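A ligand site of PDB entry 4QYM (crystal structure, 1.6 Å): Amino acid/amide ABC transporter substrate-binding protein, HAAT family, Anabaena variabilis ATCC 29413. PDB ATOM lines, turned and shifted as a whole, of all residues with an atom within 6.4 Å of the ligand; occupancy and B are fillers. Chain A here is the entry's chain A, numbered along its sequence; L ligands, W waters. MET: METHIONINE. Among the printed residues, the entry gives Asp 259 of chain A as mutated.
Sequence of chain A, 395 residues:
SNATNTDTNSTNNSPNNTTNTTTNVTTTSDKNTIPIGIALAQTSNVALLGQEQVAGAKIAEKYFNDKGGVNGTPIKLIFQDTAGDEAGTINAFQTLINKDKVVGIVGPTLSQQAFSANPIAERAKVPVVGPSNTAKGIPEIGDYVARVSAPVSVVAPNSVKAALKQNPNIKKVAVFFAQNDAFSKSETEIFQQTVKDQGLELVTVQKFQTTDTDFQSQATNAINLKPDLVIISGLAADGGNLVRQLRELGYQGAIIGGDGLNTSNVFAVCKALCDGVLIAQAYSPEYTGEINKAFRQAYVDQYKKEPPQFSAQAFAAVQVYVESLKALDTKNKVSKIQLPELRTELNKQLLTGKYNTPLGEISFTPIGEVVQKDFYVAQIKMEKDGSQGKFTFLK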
ATOM      1  N   VAL A  46      21.561   4.456  -2.225  1.00  0.00           N
ATOM      2  CA  VAL A  46      21.271   5.004  -0.916  1.00  0.00           C
ATOM      3  C   VAL A  46      22.582   5.195  -0.135  1.00  0.00           C
ATOM      4  O   VAL A  46      22.660   6.005   0.791  1.00  0.00           O
ATOM      5  CB  VAL A  46      20.273   4.093  -0.150  1.00  0.00           C
ATOM      6  CG1 VAL A  46      19.891   4.725   1.175  1.00  0.00           C
ATOM      7  CG2 VAL A  46      19.028   3.848  -1.008  1.00  0.00           C
ATOM      8  N   LEU A  49      24.073   8.518   0.611  1.00  0.00           N
ATOM      9  CA  LEU A  49      23.690   9.165   1.855  1.00  0.00           C
ATOM     10  C   LEU A  49      24.297   8.420   3.053  1.00  0.00           C
ATOM     11  O   LEU A  49      24.741   9.040   4.022  1.00  0.00           O
ATOM     12  CB  LEU A  49      22.164   9.226   1.963  1.00  0.00           C
ATOM     13  CG  LEU A  49      21.478  10.141   0.919  1.00  0.00           C
ATOM     14  CD1 LEU A  49      19.981   9.832   0.757  1.00  0.00           C
ATOM     15  CD2 LEU A  49      21.702  11.615   1.272  1.00  0.00           C
ATOM     16  N   GLY A  50      24.351   7.094   2.958  1.00  0.00           N
ATOM     17  CA  GLY A  50      24.887   6.277   4.031  1.00  0.00           C
ATOM     18  C   GLY A  50      26.374   6.482   4.288  1.00  0.00           C
ATOM     19  O   GLY A  50      26.833   6.350   5.420  1.00  0.00           O
ATOM     20  N   GLN A  53      27.417   8.711   7.034  1.00  0.00           N
ATOM     21  CA  GLN A  53      26.997   8.207   8.335  1.00  0.00           C
ATOM     22  C   GLN A  53      27.987   7.169   8.840  1.00  0.00           C
ATOM     23  O   GLN A  53      28.354   7.177  10.007  1.00  0.00           O
ATOM     24  CB  GLN A  53      25.604   7.593   8.249  1.00  0.00           C
ATOM     25  CG  GLN A  53      24.541   8.518   7.704  1.00  0.00           C
ATOM     26  CD  GLN A  53      23.213   7.818   7.648  1.00  0.00           C
ATOM     27  OE1 GLN A  53      23.058   6.819   6.946  1.00  0.00           O
ATOM     28  NE2 GLN A  53      22.247   8.300   8.410  1.00  0.00           N
ATOM     29  N   THR A 109      19.415   4.105   7.391  1.00  0.00           N
ATOM     30  CA  THR A 109      19.645   5.368   6.704  1.00  0.00           C
ATOM     31  C   THR A 109      18.356   6.119   6.363  1.00  0.00           C
ATOM     32  O   THR A 109      18.220   7.301   6.673  1.00  0.00           O
ATOM     33  CB  THR A 109      20.473   5.128   5.440  1.00  0.00           C
ATOM     34  OG1 THR A 109      21.765   4.637   5.820  1.00  0.00           O
ATOM     35  CG2 THR A 109      20.659   6.422   4.646  1.00  0.00           C
ATOM     36  N   LEU A 110      17.410   5.425   5.741  1.00  0.00           N
ATOM     37  CA  LEU A 110      16.178   6.058   5.269  1.00  0.00           C
ATOM     38  C   LEU A 110      14.966   5.827   6.159  1.00  0.00           C
ATOM     39  O   LEU A 110      14.789   4.738   6.698  1.00  0.00           O
ATOM     40  CB  LEU A 110      15.832   5.562   3.879  1.00  0.00           C
ATOM     41  CG  LEU A 110      16.860   5.847   2.793  1.00  0.00           C
ATOM     42  CD1 LEU A 110      16.325   5.252   1.501  1.00  0.00           C
ATOM     43  CD2 LEU A 110      17.102   7.345   2.654  1.00  0.00           C
ATOM     44  N   SER A 111      14.109   6.841   6.266  1.00  0.00           N
ATOM     45  CA  SER A 111      12.827   6.662   6.931  1.00  0.00           C
ATOM     46  C   SER A 111      12.030   5.561   6.268  1.00  0.00           C
ATOM     47  O   SER A 111      11.343   4.794   6.924  1.00  0.00           O
ATOM     48  CB  SER A 111      12.012   7.953   6.921  1.00  0.00           C
ATOM     49  OG  SER A 111      12.627   8.942   7.712  1.00  0.00           O
ATOM     50  N   GLN A 112      12.115   5.497   4.927  1.00  0.00           N
ATOM     51  CA  GLN A 112      11.418   4.457   4.166  1.00  0.00           C
ATOM     52  C   GLN A 112      11.775   3.074   4.678  1.00  0.00           C
ATOM     53  O   GLN A 112      10.928   2.181   4.765  1.00  0.00           O
ATOM     54  CB  GLN A 112      11.817   4.580   2.685  1.00  0.00           C
ATOM     55  CG  GLN A 112      11.230   3.487   1.792  1.00  0.00           C
ATOM     56  CD  GLN A 112       9.732   3.637   1.581  1.00  0.00           C
ATOM     57  OE1 GLN A 112       9.191   4.749   1.596  1.00  0.00           O
ATOM     58  NE2 GLN A 112       9.062   2.528   1.372  1.00  0.00           N
ATOM     59  N   SER A 132      19.349   9.737  11.154  1.00  0.00           N
ATOM     60  CA  SER A 132      18.987  10.639  10.071  1.00  0.00           C
ATOM     61  C   SER A 132      17.565  10.496   9.559  1.00  0.00           C
ATOM     62  O   SER A 132      17.239  11.033   8.498  1.00  0.00           O
ATOM     63  CB  SER A 132      19.920  10.382   8.891  1.00  0.00           C
ATOM     64  OG  SER A 132      19.792   9.032   8.469  1.00  0.00           O
ATOM     65  N   ASN A 133      16.728   9.721  10.254  1.00  0.00           N
ATOM     66  CA  ASN A 133      15.349   9.478   9.785  1.00  0.00           C
ATOM     67  C   ASN A 133      14.437  10.602  10.246  1.00  0.00           C
ATOM     68  O   ASN A 133      14.123  10.687  11.425  1.00  0.00           O
ATOM     69  CB  ASN A 133      14.766   8.183  10.361  1.00  0.00           C
ATOM     70  CG  ASN A 133      15.696   7.013  10.254  1.00  0.00           C
ATOM     71  OD1 ASN A 133      15.822   6.230  11.193  1.00  0.00           O
ATOM     72  ND2 ASN A 133      16.325   6.840   9.096  1.00  0.00           N
ATOM     73  N   THR A 134      13.973  11.432   9.311  1.00  0.00           N
ATOM     74  CA  THR A 134      13.302  12.678   9.693  1.00  0.00           C
ATOM     75  C   THR A 134      11.834  12.743   9.290  1.00  0.00           C
ATOM     76  O   THR A 134      11.180  13.767   9.499  1.00  0.00           O
ATOM     77  CB  THR A 134      14.047  13.906   9.142  1.00  0.00           C
ATOM     78  OG1 THR A 134      14.110  13.837   7.709  1.00  0.00           O
ATOM     79  CG2 THR A 134      15.472  13.963   9.692  1.00  0.00           C
ATOM     80  N   ALA A 135      11.299  11.656   8.753  1.00  0.00           N
ATOM     81  CA  ALA A 135       9.871  11.586   8.445  1.00  0.00           C
ATOM     82  C   ALA A 135       9.006  11.677   9.717  1.00  0.00           C
ATOM     83  O   ALA A 135       9.392  11.207  10.781  1.00  0.00           O
ATOM     84  CB  ALA A 135       9.542  10.321   7.673  1.00  0.00           C
ATOM     85  N   ILE A 138       8.352   8.548  13.066  1.00  0.00           N
ATOM     86  CA  ILE A 138       9.392   7.573  13.388  1.00  0.00           C
ATOM     87  C   ILE A 138       9.436   7.146  14.881  1.00  0.00           C
ATOM     88  O   ILE A 138       9.338   5.962  15.173  1.00  0.00           O
ATOM     89  CB  ILE A 138      10.790   8.021  12.854  1.00  0.00           C
ATOM     90  CG1 ILE A 138      10.794   8.076  11.329  1.00  0.00           C
ATOM     91  CG2 ILE A 138      11.887   7.105  13.389  1.00  0.00           C
ATOM     92  CD1 ILE A 138      10.865   6.727  10.684  1.00  0.00           C
ATOM     93  N   SER A 149      17.826  12.760  15.057  1.00  0.00           N
ATOM     94  CA  SER A 149      17.648  13.655  13.928  1.00  0.00           C
ATOM     95  C   SER A 149      16.307  14.383  13.976  1.00  0.00           C
ATOM     96  O   SER A 149      15.249  13.757  13.821  1.00  0.00           O
ATOM     97  CB  SER A 149      17.741  12.872  12.630  1.00  0.00           C
ATOM     98  OG  SER A 149      16.857  11.749  12.669  1.00  0.00           O
ATOM     99  N   VAL A 152      11.268  16.692   9.786  1.00  0.00           N
ATOM    100  CA  VAL A 152      11.068  17.648   8.703  1.00  0.00           C
ATOM    101  C   VAL A 152      10.304  18.905   9.132  1.00  0.00           C
ATOM    102  O   VAL A 152      10.574  20.000   8.647  1.00  0.00           O
ATOM    103  CB  VAL A 152      10.372  16.985   7.492  1.00  0.00           C
ATOM    104  CG1 VAL A 152      11.312  15.985   6.829  1.00  0.00           C
ATOM    105  CG2 VAL A 152       9.074  16.289   7.916  1.00  0.00           C
ATOM    106  N   ASP A 181       9.027   7.583  -1.814  1.00  0.00           N
ATOM    107  CA  ASP A 181       9.857   7.653  -0.621  1.00  0.00           C
ATOM    108  C   ASP A 181       9.147   8.295   0.570  1.00  0.00           C
ATOM    109  O   ASP A 181       8.670   9.428   0.477  1.00  0.00           O
ATOM    110  CB  ASP A 181      11.155   8.408  -0.930  1.00  0.00           C
ATOM    111  CG  ASP A 181      12.040   8.536   0.294  1.00  0.00           C
ATOM    112  OD1 ASP A 181      12.681   7.540   0.680  1.00  0.00           O
ATOM    113  OD2 ASP A 181      12.091   9.653   0.871  1.00  0.00           O
ATOM    114  N   PHE A 183      10.063   9.574   3.513  1.00  0.00           N
ATOM    115  CA  PHE A 183      10.567  10.853   3.986  1.00  0.00           C
ATOM    116  C   PHE A 183      10.239  11.996   3.008  1.00  0.00           C
ATOM    117  O   PHE A 183       9.860  13.081   3.436  1.00  0.00           O
ATOM    118  CB  PHE A 183      12.070  10.778   4.243  1.00  0.00           C
ATOM    119  CG  PHE A 183      12.811  12.036   3.883  1.00  0.00           C
ATOM    120  CD1 PHE A 183      12.864  13.120   4.751  1.00  0.00           C
ATOM    121  CD2 PHE A 183      13.479  12.129   2.657  1.00  0.00           C
ATOM    122  CE1 PHE A 183      13.542  14.270   4.417  1.00  0.00           C
ATOM    123  CE2 PHE A 183      14.160  13.281   2.314  1.00  0.00           C
ATOM    124  CZ  PHE A 183      14.200  14.356   3.197  1.00  0.00           C
ATOM    125  N   SER A 184      10.383  11.749   1.708  1.00  0.00           N
ATOM    126  CA  SER A 184      10.124  12.781   0.721  1.00  0.00           C
ATOM    127  C   SER A 184       8.660  13.244   0.777  1.00  0.00           C
ATOM    128  O   SER A 184       8.370  14.443   0.629  1.00  0.00           O
ATOM    129  CB  SER A 184      10.474  12.287  -0.696  1.00  0.00           C
ATOM    130  OG  SER A 184      11.864  12.002  -0.808  1.00  0.00           O
ATOM    131  N   LEU A 235      15.956  12.062  -2.922  1.00  0.00           N
ATOM    132  CA  LEU A 235      17.251  11.649  -2.399  1.00  0.00           C
ATOM    133  C   LEU A 235      18.385  12.225  -3.262  1.00  0.00           C
ATOM    134  O   LEU A 235      18.157  13.161  -4.025  1.00  0.00           O
ATOM    135  CB  LEU A 235      17.317  10.132  -2.251  1.00  0.00           C
ATOM    136  CG  LEU A 235      16.207   9.573  -1.345  1.00  0.00           C
ATOM    137  CD1 LEU A 235      16.297   8.051  -1.226  1.00  0.00           C
ATOM    138  CD2 LEU A 235      16.239  10.223   0.035  1.00  0.00           C
ATOM    139  N   ASP A 259      16.409  17.333   2.730  1.00  0.00           N
ATOM    140  CA  ASP A 259      17.473  16.642   3.446  1.00  0.00           C
ATOM    141  C   ASP A 259      18.115  15.535   2.619  1.00  0.00           C
ATOM    142  O   ASP A 259      19.265  15.169   2.846  1.00  0.00           O
ATOM    143  CB  ASP A 259      16.932  16.080   4.767  1.00  0.00           C
ATOM    144  CG  ASP A 259      18.028  15.789   5.766  1.00  0.00           C
ATOM    145  OD1 ASP A 259      18.873  16.675   6.009  1.00  0.00           O
ATOM    146  OD2 ASP A 259      18.053  14.679   6.323  1.00  0.00           O
ATOM    147  N   GLY A 260      17.370  15.020   1.637  1.00  0.00           N
ATOM    148  CA  GLY A 260      17.901  13.973   0.783  1.00  0.00           C
ATOM    149  C   GLY A 260      18.948  14.432  -0.201  1.00  0.00           C
ATOM    150  O   GLY A 260      19.656  13.614  -0.783  1.00  0.00           O
ATOM    151  N   GLN A 309      26.407  17.187   8.063  1.00  0.00           N
ATOM    152  CA  GLN A 309      25.345  16.843   9.004  1.00  0.00           C
ATOM    153  C   GLN A 309      25.204  15.354   9.265  1.00  0.00           C
ATOM    154  O   GLN A 309      25.095  14.935  10.405  1.00  0.00           O
ATOM    155  CB  GLN A 309      24.032  17.428   8.499  1.00  0.00           C
ATOM    156  CG  GLN A 309      22.821  17.027   9.315  1.00  0.00           C
ATOM    157  CD  GLN A 309      21.535  17.334   8.589  1.00  0.00           C
ATOM    158  OE1 GLN A 309      21.092  18.475   8.549  1.00  0.00           O
ATOM    159  NE2 GLN A 309      20.946  16.311   7.985  1.00  0.00           N
ATOM    160  N   PHE A 310      25.189  14.534   8.210  1.00  0.00           N
ATOM    161  CA  PHE A 310      24.957  13.102   8.393  1.00  0.00           C
ATOM    162  C   PHE A 310      26.051  12.419   9.205  1.00  0.00           C
ATOM    163  O   PHE A 310      25.784  11.461   9.947  1.00  0.00           O
ATOM    164  CB  PHE A 310      24.766  12.393   7.045  1.00  0.00           C
ATOM    165  CG  PHE A 310      23.532  12.809   6.322  1.00  0.00           C
ATOM    166  CD1 PHE A 310      22.338  12.997   7.005  1.00  0.00           C
ATOM    167  CD2 PHE A 310      23.552  13.004   4.952  1.00  0.00           C
ATOM    168  CE1 PHE A 310      21.186  13.381   6.323  1.00  0.00           C
ATOM    169  CE2 PHE A 310      22.413  13.383   4.271  1.00  0.00           C
ATOM    170  CZ  PHE A 310      21.227  13.576   4.957  1.00  0.00           C
ATOM    171  N   GLN A 313      25.435  13.474  12.883  1.00  0.00           N
ATOM    172  CA  GLN A 313      24.258  12.797  13.426  1.00  0.00           C
ATOM    173  C   GLN A 313      24.550  11.344  13.762  1.00  0.00           C
ATOM    174  O   GLN A 313      24.098  10.830  14.786  1.00  0.00           O
ATOM    175  CB  GLN A 313      23.090  12.929  12.446  1.00  0.00           C
ATOM    176  CG  GLN A 313      22.468  14.308  12.463  1.00  0.00           C
ATOM    177  CD  GLN A 313      21.365  14.461  11.440  1.00  0.00           C
ATOM    178  OE1 GLN A 313      21.431  13.903  10.336  1.00  0.00           O
ATOM    179  NE2 GLN A 313      20.347  15.239  11.780  1.00  0.00           N
HETATM  180  N   MET L   1      16.282  12.451   6.416  1.00  0.00           N
HETATM  181  CA  MET L   1      15.944  11.639   5.249  1.00  0.00           C
HETATM  182  C   MET L   1      15.122  10.429   5.671  1.00  0.00           C
HETATM  183  O   MET L   1      15.044   9.414   4.970  1.00  0.00           O
HETATM  184  CB  MET L   1      17.198  11.209   4.493  1.00  0.00           C
HETATM  185  CG  MET L   1      18.296  10.623   5.357  1.00  0.00           C
HETATM  186  SD  MET L   1      19.696  10.153   4.320  1.00  0.00           S
HETATM  187  CE  MET L   1      20.970   9.889   5.561  1.00  0.00           C
HETATM  188  OXT MET L   1      14.501  10.463   6.733  1.00  0.00           O
HETATM  189  O   HOH W   1      13.093   7.724   3.327  1.00  0.00           O
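The side-chain amide nitrogen (ND2) of Asn 133 is in hydrogen-bond range of the backbone carbonyl oxygen (O) of Thr 109, at 3.1 Å.
OG of Ser 111 is in hydrogen-bond range of N of Thr 134, 3.3 Å away.
OD1 of Asp 259 lies within hydrogen-bond range of NE2 of Gln 309 (2.9 Å).
The backbone carbonyl oxygen (O) of Thr 134 lies within hydrogen-bond range of the backbone NH (N) of Val 152.
The side-chain hydroxyl (OG) of Ser 132 lies within hydrogen-bond range of the backbone carbonyl oxygen (O) of Thr 109.
The side-chain hydroxyl (OG) of Ser 132 sits at hydrogen-bond distance from the side-chain amide nitrogen (NE2) of Gln 53 (2.6 Å).
OD2 of Asp 181 lies within hydrogen-bond range of N of Phe 183 (3.3 Å).
The side-chain hydroxyl (OG) of Ser 149 lies within hydrogen-bond range of the backbone NH (N) of Asn 133 (3.2 Å).
O of the ligand is in hydrogen-bond range of N of Ser 111, 3.0 Å away.
The backbone NH of Thr 134 lies within hydrogen-bond range of an oxygen (OXT) of the ligand (2.8 Å).
N of the ligand lies within hydrogen-bond range of OG1 of Thr 134 (2.9 Å).
N of the ligand lies within salt-bridge range of OD2 of Asp 259.
O of Ser 132 lies within hydrogen-bond range of N of the ligand.
The side-chain hydroxyl (OG) of Ser 111 lies within hydrogen-bond range of an oxygen (OXT) of the ligand (2.6 Å).
Water W1 lies within hydrogen-bond range of the side-chain carboxylate of Asp 181 (2.7 Å), the backbone NH of Gln 112 (2.9 Å), an oxygen (O) of the ligand (3.1 Å) and the backbone NH of Ser 111 (3.2 Å).
Merely in contact with the ligand: Asn 133, Phe 183, Gln 53, Leu 49, Leu 110, Thr 109, Phe 310 and Ala 135.
Hydrophobic or aromatic side chains that line the ligand: Leu 49, Leu 110, Phe 183 and Phe 310.
Within 4 Å of the ligand: Leu 49, Gln 53, Thr 109, Leu 110, Ser 111, Ser 132, Asn 133, Thr 134, Ala 135, Phe 183, Asp 259 and Phe 310.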
